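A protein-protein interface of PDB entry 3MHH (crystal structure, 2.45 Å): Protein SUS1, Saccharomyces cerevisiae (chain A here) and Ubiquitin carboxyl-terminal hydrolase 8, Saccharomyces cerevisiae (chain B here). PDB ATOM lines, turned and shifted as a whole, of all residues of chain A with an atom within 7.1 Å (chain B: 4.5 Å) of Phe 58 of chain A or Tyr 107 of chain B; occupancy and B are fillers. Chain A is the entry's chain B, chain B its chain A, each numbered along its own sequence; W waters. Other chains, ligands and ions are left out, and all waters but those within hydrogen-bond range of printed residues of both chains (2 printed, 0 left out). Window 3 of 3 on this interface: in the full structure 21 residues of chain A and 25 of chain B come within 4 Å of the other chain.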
ATOM      1  N   SER A  55      25.561  -7.555 -36.906  1.00  0.00           N
ATOM      2  CA  SER A  55      25.935  -8.656 -36.036  1.00  0.00           C
ATOM      3  C   SER A  55      24.805  -9.013 -35.077  1.00  0.00           C
ATOM      4  O   SER A  55      24.004  -8.161 -34.693  1.00  0.00           O
ATOM      5  CB  SER A  55      27.190  -8.272 -35.249  1.00  0.00           C
ATOM      6  OG  SER A  55      27.357  -9.074 -34.087  1.00  0.00           O
ATOM      7  N   THR A  56      24.739 -10.283 -34.693  1.00  0.00           N
ATOM      8  CA  THR A  56      23.858 -10.696 -33.613  1.00  0.00           C
ATOM      9  C   THR A  56      24.675 -11.239 -32.444  1.00  0.00           C
ATOM     10  O   THR A  56      24.110 -11.812 -31.503  1.00  0.00           O
ATOM     11  CB  THR A  56      22.875 -11.781 -34.072  1.00  0.00           C
ATOM     12  OG1 THR A  56      23.607 -12.882 -34.631  1.00  0.00           O
ATOM     13  CG2 THR A  56      21.919 -11.223 -35.114  1.00  0.00           C
ATOM     14  N   ASN A  57      26.001 -11.089 -32.513  1.00  0.00           N
ATOM     15  CA  ASN A  57      26.880 -11.535 -31.425  1.00  0.00           C
ATOM     16  C   ASN A  57      26.569 -10.801 -30.123  1.00  0.00           C
ATOM     17  O   ASN A  57      26.767  -9.590 -30.020  1.00  0.00           O
ATOM     18  CB  ASN A  57      28.359 -11.333 -31.784  1.00  0.00           C
ATOM     19  CG  ASN A  57      29.303 -11.821 -30.682  1.00  0.00           C
ATOM     20  OD1 ASN A  57      29.952 -12.863 -30.818  1.00  0.00           O
ATOM     21  ND2 ASN A  57      29.364 -11.083 -29.579  1.00  0.00           N
ATOM     22  N   PHE A  58      26.119 -11.548 -29.124  1.00  0.00           N
ATOM     23  CA  PHE A  58      25.676 -10.971 -27.869  1.00  0.00           C
ATOM     24  C   PHE A  58      26.653 -10.029 -27.173  1.00  0.00           C
ATOM     25  O   PHE A  58      26.285  -8.931 -26.756  1.00  0.00           O
ATOM     26  CB  PHE A  58      25.306 -12.061 -26.867  1.00  0.00           C
ATOM     27  CG  PHE A  58      24.874 -11.501 -25.559  1.00  0.00           C
ATOM     28  CD1 PHE A  58      23.617 -10.944 -25.424  1.00  0.00           C
ATOM     29  CD2 PHE A  58      25.761 -11.407 -24.502  1.00  0.00           C
ATOM     30  CE1 PHE A  58      23.226 -10.382 -24.250  1.00  0.00           C
ATOM     31  CE2 PHE A  58      25.375 -10.824 -23.310  1.00  0.00           C
ATOM     32  CZ  PHE A  58      24.113 -10.309 -23.188  1.00  0.00           C
ATOM     33  N   THR A  59      27.874 -10.499 -26.975  1.00  0.00           N
ATOM     34  CA  THR A  59      28.891  -9.736 -26.269  1.00  0.00           C
ATOM     35  C   THR A  59      29.111  -8.396 -26.955  1.00  0.00           C
ATOM     36  O   THR A  59      29.099  -7.338 -26.316  1.00  0.00           O
ATOM     37  CB  THR A  59      30.211 -10.511 -26.257  1.00  0.00           C
ATOM     38  OG1 THR A  59      30.007 -11.765 -25.598  1.00  0.00           O
ATOM     39  CG2 THR A  59      31.299  -9.725 -25.538  1.00  0.00           C
ATOM     40  N   GLN A  60      29.303  -8.459 -28.263  1.00  0.00           N
ATOM     41  CA  GLN A  60      29.487  -7.273 -29.072  1.00  0.00           C
ATOM     42  C   GLN A  60      28.293  -6.339 -28.926  1.00  0.00           C
ATOM     43  O   GLN A  60      28.453  -5.150 -28.652  1.00  0.00           O
ATOM     44  CB  GLN A  60      29.657  -7.673 -30.541  1.00  0.00           C
ATOM     45  CG  GLN A  60      30.169  -6.573 -31.439  1.00  0.00           C
ATOM     46  CD  GLN A  60      30.091  -6.938 -32.919  1.00  0.00           C
ATOM     47  OE1 GLN A  60      30.027  -6.061 -33.780  1.00  0.00           O
ATOM     48  NE2 GLN A  60      30.089  -8.235 -33.216  1.00  0.00           N
ATOM     49  N   ILE A  61      27.095  -6.876 -29.108  1.00  0.00           N
ATOM     50  CA  ILE A  61      25.907  -6.042 -29.095  1.00  0.00           C
ATOM     51  C   ILE A  61      25.680  -5.446 -27.709  1.00  0.00           C
ATOM     52  O   ILE A  61      25.359  -4.271 -27.576  1.00  0.00           O
ATOM     53  CB  ILE A  61      24.671  -6.820 -29.579  1.00  0.00           C
ATOM     54  CG1 ILE A  61      24.860  -7.207 -31.033  1.00  0.00           C
ATOM     55  CG2 ILE A  61      23.417  -5.977 -29.454  1.00  0.00           C
ATOM     56  CD1 ILE A  61      25.252  -6.030 -31.897  1.00  0.00           C
ATOM     57  N   LEU A  62      25.901  -6.244 -26.674  1.00  0.00           N
ATOM     58  CA  LEU A  62      25.689  -5.770 -25.310  1.00  0.00           C
ATOM     59  C   LEU A  62      26.515  -4.515 -25.039  1.00  0.00           C
ATOM     60  O   LEU A  62      26.028  -3.560 -24.438  1.00  0.00           O
ATOM     61  CB  LEU A  62      26.026  -6.864 -24.286  1.00  0.00           C
ATOM     62  CG  LEU A  62      25.867  -6.454 -22.819  1.00  0.00           C
ATOM     63  CD1 LEU A  62      24.405  -6.203 -22.488  1.00  0.00           C
ATOM     64  CD2 LEU A  62      26.466  -7.501 -21.872  1.00  0.00           C
ATOM     65  N   SER A  63      27.753  -4.510 -25.520  1.00  0.00           N
ATOM     66  CA  SER A  63      28.696  -3.437 -25.217  1.00  0.00           C
ATOM     67  C   SER A  63      28.299  -2.079 -25.795  1.00  0.00           C
ATOM     68  O   SER A  63      28.803  -1.053 -25.348  1.00  0.00           O
ATOM     69  CB  SER A  63      30.095  -3.813 -25.707  1.00  0.00           C
ATOM     70  OG  SER A  63      30.095  -3.987 -27.112  1.00  0.00           O
ATOM     71  N   THR A  64      27.415  -2.062 -26.789  1.00  0.00           N
ATOM     72  CA  THR A  64      26.956  -0.794 -27.354  1.00  0.00           C
ATOM     73  C   THR A  64      25.580  -0.421 -26.825  1.00  0.00           C
ATOM     74  O   THR A  64      25.220   0.755 -26.788  1.00  0.00           O
ATOM     75  CB  THR A  64      26.916  -0.821 -28.894  1.00  0.00           C
ATOM     76  OG1 THR A  64      26.239  -2.001 -29.344  1.00  0.00           O
ATOM     77  CG2 THR A  64      28.329  -0.788 -29.462  1.00  0.00           C
ATOM     78  N   PHE B  63      24.642 -17.447 -14.747  1.00  0.00           N
ATOM     79  CA  PHE B  63      24.549 -18.611 -15.623  1.00  0.00           C
ATOM     80  C   PHE B  63      24.642 -19.927 -14.872  1.00  0.00           C
ATOM     81  O   PHE B  63      25.483 -20.099 -14.008  1.00  0.00           O
ATOM     82  CB  PHE B  63      25.620 -18.542 -16.697  1.00  0.00           C
ATOM     83  CG  PHE B  63      25.495 -17.346 -17.585  1.00  0.00           C
ATOM     84  CD1 PHE B  63      24.773 -17.416 -18.758  1.00  0.00           C
ATOM     85  CD2 PHE B  63      26.080 -16.144 -17.232  1.00  0.00           C
ATOM     86  CE1 PHE B  63      24.650 -16.316 -19.578  1.00  0.00           C
ATOM     87  CE2 PHE B  63      25.961 -15.043 -18.043  1.00  0.00           C
ATOM     88  CZ  PHE B  63      25.245 -15.126 -19.221  1.00  0.00           C
ATOM     89  N   TRP B  74      27.967 -12.522 -14.777  1.00  0.00           N
ATOM     90  CA  TRP B  74      28.506 -11.910 -15.978  1.00  0.00           C
ATOM     91  C   TRP B  74      29.396 -10.733 -15.632  1.00  0.00           C
ATOM     92  O   TRP B  74      30.532 -10.637 -16.100  1.00  0.00           O
ATOM     93  CB  TRP B  74      27.358 -11.405 -16.844  1.00  0.00           C
ATOM     94  CG  TRP B  74      27.805 -10.656 -18.048  1.00  0.00           C
ATOM     95  CD1 TRP B  74      28.014  -9.313 -18.147  1.00  0.00           C
ATOM     96  CD2 TRP B  74      28.097 -11.206 -19.336  1.00  0.00           C
ATOM     97  NE1 TRP B  74      28.419  -8.991 -19.415  1.00  0.00           N
ATOM     98  CE2 TRP B  74      28.472 -10.133 -20.169  1.00  0.00           C
ATOM     99  CE3 TRP B  74      28.071 -12.500 -19.869  1.00  0.00           C
ATOM    100  CZ2 TRP B  74      28.826 -10.312 -21.508  1.00  0.00           C
ATOM    101  CZ3 TRP B  74      28.419 -12.678 -21.203  1.00  0.00           C
ATOM    102  CH2 TRP B  74      28.792 -11.589 -22.005  1.00  0.00           C
ATOM    103  N   ASN B  93      21.394 -18.789 -18.840  1.00  0.00           N
ATOM    104  CA  ASN B  93      20.980 -17.549 -18.204  1.00  0.00           C
ATOM    105  C   ASN B  93      19.703 -17.770 -17.391  1.00  0.00           C
ATOM    106  O   ASN B  93      18.669 -18.143 -17.932  1.00  0.00           O
ATOM    107  CB  ASN B  93      20.781 -16.472 -19.283  1.00  0.00           C
ATOM    108  CG  ASN B  93      20.295 -15.158 -18.720  1.00  0.00           C
ATOM    109  OD1 ASN B  93      19.500 -15.131 -17.784  1.00  0.00           O
ATOM    110  ND2 ASN B  93      20.762 -14.056 -19.298  1.00  0.00           N
ATOM    111  N   LEU B  98      18.205 -19.197 -21.821  1.00  0.00           N
ATOM    112  CA  LEU B  98      18.988 -19.249 -23.052  1.00  0.00           C
ATOM    113  C   LEU B  98      20.362 -19.808 -22.761  1.00  0.00           C
ATOM    114  O   LEU B  98      20.946 -19.553 -21.701  1.00  0.00           O
ATOM    115  CB  LEU B  98      19.125 -17.866 -23.685  1.00  0.00           C
ATOM    116  CG  LEU B  98      17.822 -17.180 -24.110  1.00  0.00           C
ATOM    117  CD1 LEU B  98      18.094 -15.722 -24.467  1.00  0.00           C
ATOM    118  CD2 LEU B  98      17.152 -17.936 -25.265  1.00  0.00           C
ATOM    119  N   LEU B  99      20.884 -20.567 -23.717  1.00  0.00           N
ATOM    120  CA  LEU B  99      22.124 -21.298 -23.529  1.00  0.00           C
ATOM    121  C   LEU B  99      23.251 -20.468 -24.106  1.00  0.00           C
ATOM    122  O   LEU B  99      23.143 -19.988 -25.227  1.00  0.00           O
ATOM    123  CB  LEU B  99      22.030 -22.633 -24.248  1.00  0.00           C
ATOM    124  CG  LEU B  99      23.192 -23.597 -24.086  1.00  0.00           C
ATOM    125  CD1 LEU B  99      23.334 -24.012 -22.620  1.00  0.00           C
ATOM    126  CD2 LEU B  99      22.942 -24.789 -24.983  1.00  0.00           C
ATOM    127  N   PHE B 100      24.313 -20.274 -23.331  1.00  0.00           N
ATOM    128  CA  PHE B 100      25.422 -19.436 -23.761  1.00  0.00           C
ATOM    129  C   PHE B 100      26.680 -20.261 -23.940  1.00  0.00           C
ATOM    130  O   PHE B 100      26.939 -21.193 -23.186  1.00  0.00           O
ATOM    131  CB  PHE B 100      25.695 -18.344 -22.731  1.00  0.00           C
ATOM    132  CG  PHE B 100      26.574 -17.236 -23.238  1.00  0.00           C
ATOM    133  CD1 PHE B 100      26.026 -16.168 -23.929  1.00  0.00           C
ATOM    134  CD2 PHE B 100      27.940 -17.236 -22.980  1.00  0.00           C
ATOM    135  CE1 PHE B 100      26.814 -15.144 -24.390  1.00  0.00           C
ATOM    136  CE2 PHE B 100      28.737 -16.196 -23.421  1.00  0.00           C
ATOM    137  CZ  PHE B 100      28.167 -15.147 -24.129  1.00  0.00           C
ATOM    138  N   ASP B 106      28.844 -16.036 -27.270  1.00  0.00           N
ATOM    139  CA  ASP B 106      27.527 -15.706 -27.801  1.00  0.00           C
ATOM    140  C   ASP B 106      26.479 -16.756 -27.422  1.00  0.00           C
ATOM    141  O   ASP B 106      26.823 -17.879 -27.057  1.00  0.00           O
ATOM    142  CB  ASP B 106      27.591 -15.583 -29.321  1.00  0.00           C
ATOM    143  CG  ASP B 106      26.350 -14.946 -29.907  1.00  0.00           C
ATOM    144  OD1 ASP B 106      25.685 -14.145 -29.204  1.00  0.00           O
ATOM    145  OD2 ASP B 106      26.042 -15.243 -31.075  1.00  0.00           O
ATOM    146  N   TYR B 107      25.203 -16.388 -27.514  1.00  0.00           N
ATOM    147  CA  TYR B 107      24.131 -17.325 -27.231  1.00  0.00           C
ATOM    148  C   TYR B 107      23.981 -18.272 -28.410  1.00  0.00           C
ATOM    149  O   TYR B 107      24.246 -17.901 -29.541  1.00  0.00           O
ATOM    150  CB  TYR B 107      22.802 -16.593 -26.936  1.00  0.00           C
ATOM    151  CG  TYR B 107      22.712 -16.077 -25.517  1.00  0.00           C
ATOM    152  CD1 TYR B 107      22.412 -16.930 -24.460  1.00  0.00           C
ATOM    153  CD2 TYR B 107      22.994 -14.748 -25.223  1.00  0.00           C
ATOM    154  CE1 TYR B 107      22.368 -16.465 -23.155  1.00  0.00           C
ATOM    155  CE2 TYR B 107      22.962 -14.277 -23.931  1.00  0.00           C
ATOM    156  CZ  TYR B 107      22.651 -15.135 -22.900  1.00  0.00           C
ATOM    157  OH  TYR B 107      22.626 -14.650 -21.613  1.00  0.00           O
ATOM    158  N   ILE B 108      23.606 -19.509 -28.117  1.00  0.00           N
ATOM    159  CA  ILE B 108      23.261 -20.486 -29.136  1.00  0.00           C
ATOM    160  C   ILE B 108      21.761 -20.395 -29.317  1.00  0.00           C
ATOM    161  O   ILE B 108      20.986 -20.960 -28.531  1.00  0.00           O
ATOM    162  CB  ILE B 108      23.640 -21.909 -28.676  1.00  0.00           C
ATOM    163  CG1 ILE B 108      25.160 -22.011 -28.483  1.00  0.00           C
ATOM    164  CG2 ILE B 108      23.172 -22.927 -29.670  1.00  0.00           C
ATOM    165  CD1 ILE B 108      25.607 -23.202 -27.666  1.00  0.00           C
ATOM    166  N   GLY B 109      21.343 -19.627 -30.313  1.00  0.00           N
ATOM    167  CA  GLY B 109      19.934 -19.309 -30.474  1.00  0.00           C
ATOM    168  C   GLY B 109      19.317 -19.859 -31.740  1.00  0.00           C
ATOM    169  O   GLY B 109      18.106 -19.818 -31.902  1.00  0.00           O
HETATM  170  O   HOH W   1      23.222 -13.928 -29.091  1.00  0.00           O
HETATM  171  O   HOH W   2      24.304 -14.173 -32.548  1.00  0.00           O
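Printed residues of chain A that touch a printed residue of chain B: Thr 56, Asn 57, Phe 58, Thr 59 and Leu 62. Hydrophobic or aromatic side chains of chain B within 4 Å of the printed part of chain A: Trp 74, Phe 100 and Tyr 107. Along chain B the printed residues that touch a printed residue of chain A span positions 74 to 107. Among the printed residues, no Asp or Glu carboxylate lies within 4 Å of a Lys or Arg side-chain nitrogen of the other chain.
Water W1 bridges the side-chain carboxylate of Asp 106 of chain B (2.5 Å) and the backbone carbonyl oxygen of Thr 56 of chain A (3.3 Å). Water W2 bridges OD2 of Asp 106 of chain B (2.5 Å) and OG1 of Thr 56 of chain A (2.5 Å).
Among the printed residues, merely in contact across the chains: Leu 62 of chain A with Trp 74 of chain B (3.5 Å), Asn 57 of chain A with Asp 106 of chain B (3.6 Å), Thr 56 of chain A with Asp 106 of chain B (3.6 Å), Phe 58 of chain A with Tyr 107 of chain B (3.7 Å), Phe 58 of chain A with Trp 74 of chain B (3.7 Å), Thr 59 of chain A with Trp 74 of chain B (3.8 Å) and Phe 58 of chain A with Phe 100 of chain B (3.9 Å).
Phe 58 of chain A touches just these residues of chain B: Trp 74 (3.7 Å), Phe 100 (3.9 Å), Asp 106 (2.6 Å) and Tyr 107 (3.7 Å). Of chain A, only Phe 58 (3.7 Å) comes within 4 Å of Tyr 107 of chain B. Printed residues of chain A within 4 Å of Trp 74 of chain B: Phe 58 (3.7 Å), Thr 59 (3.8 Å) and Leu 62 (3.5 Å). Printed residues of chain B within 4 Å of Asn 57 of chain A: Asp 106 (3.6 Å). Printed residues of chain B within 4 Å of Leu 62 of chain A: Trp 74. Of the printed residues of chain B, Thr 59 of chain A touches Trp 74. The nearest printed residue of chain B that does not touch Phe 58 of chain A is Phe 63 of chain B (5.9 Å). The nearest residue of chain A that does not touch Tyr 107 of chain B is Thr 56 of chain A (6.2 Å).
The backbone NH (N) of Phe 58 of chain A sits at hydrogen-bond distance from the side-chain carboxylate (OD1) of Asp 106 of chain B, 2.6 Å away.
The backbone NH of Gln 60 of chain A lies close to the side-chain amide nitrogen of Asn 57 of chain A (2.9 Å). The side-chain amide nitrogen (ND2) of Asn 93 of chain B sits at hydrogen-bond distance from the side-chain hydroxyl (OH) of Tyr 107 of chain B, at 3.0 Å. OG of Ser 55 of chain A is in hydrogen-bond range of N of Asn 57 of chain A (2.9 Å). ND2 of Asn 57 of chain A sits close to N of Thr 59 of chain A, 3.1 Å away.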
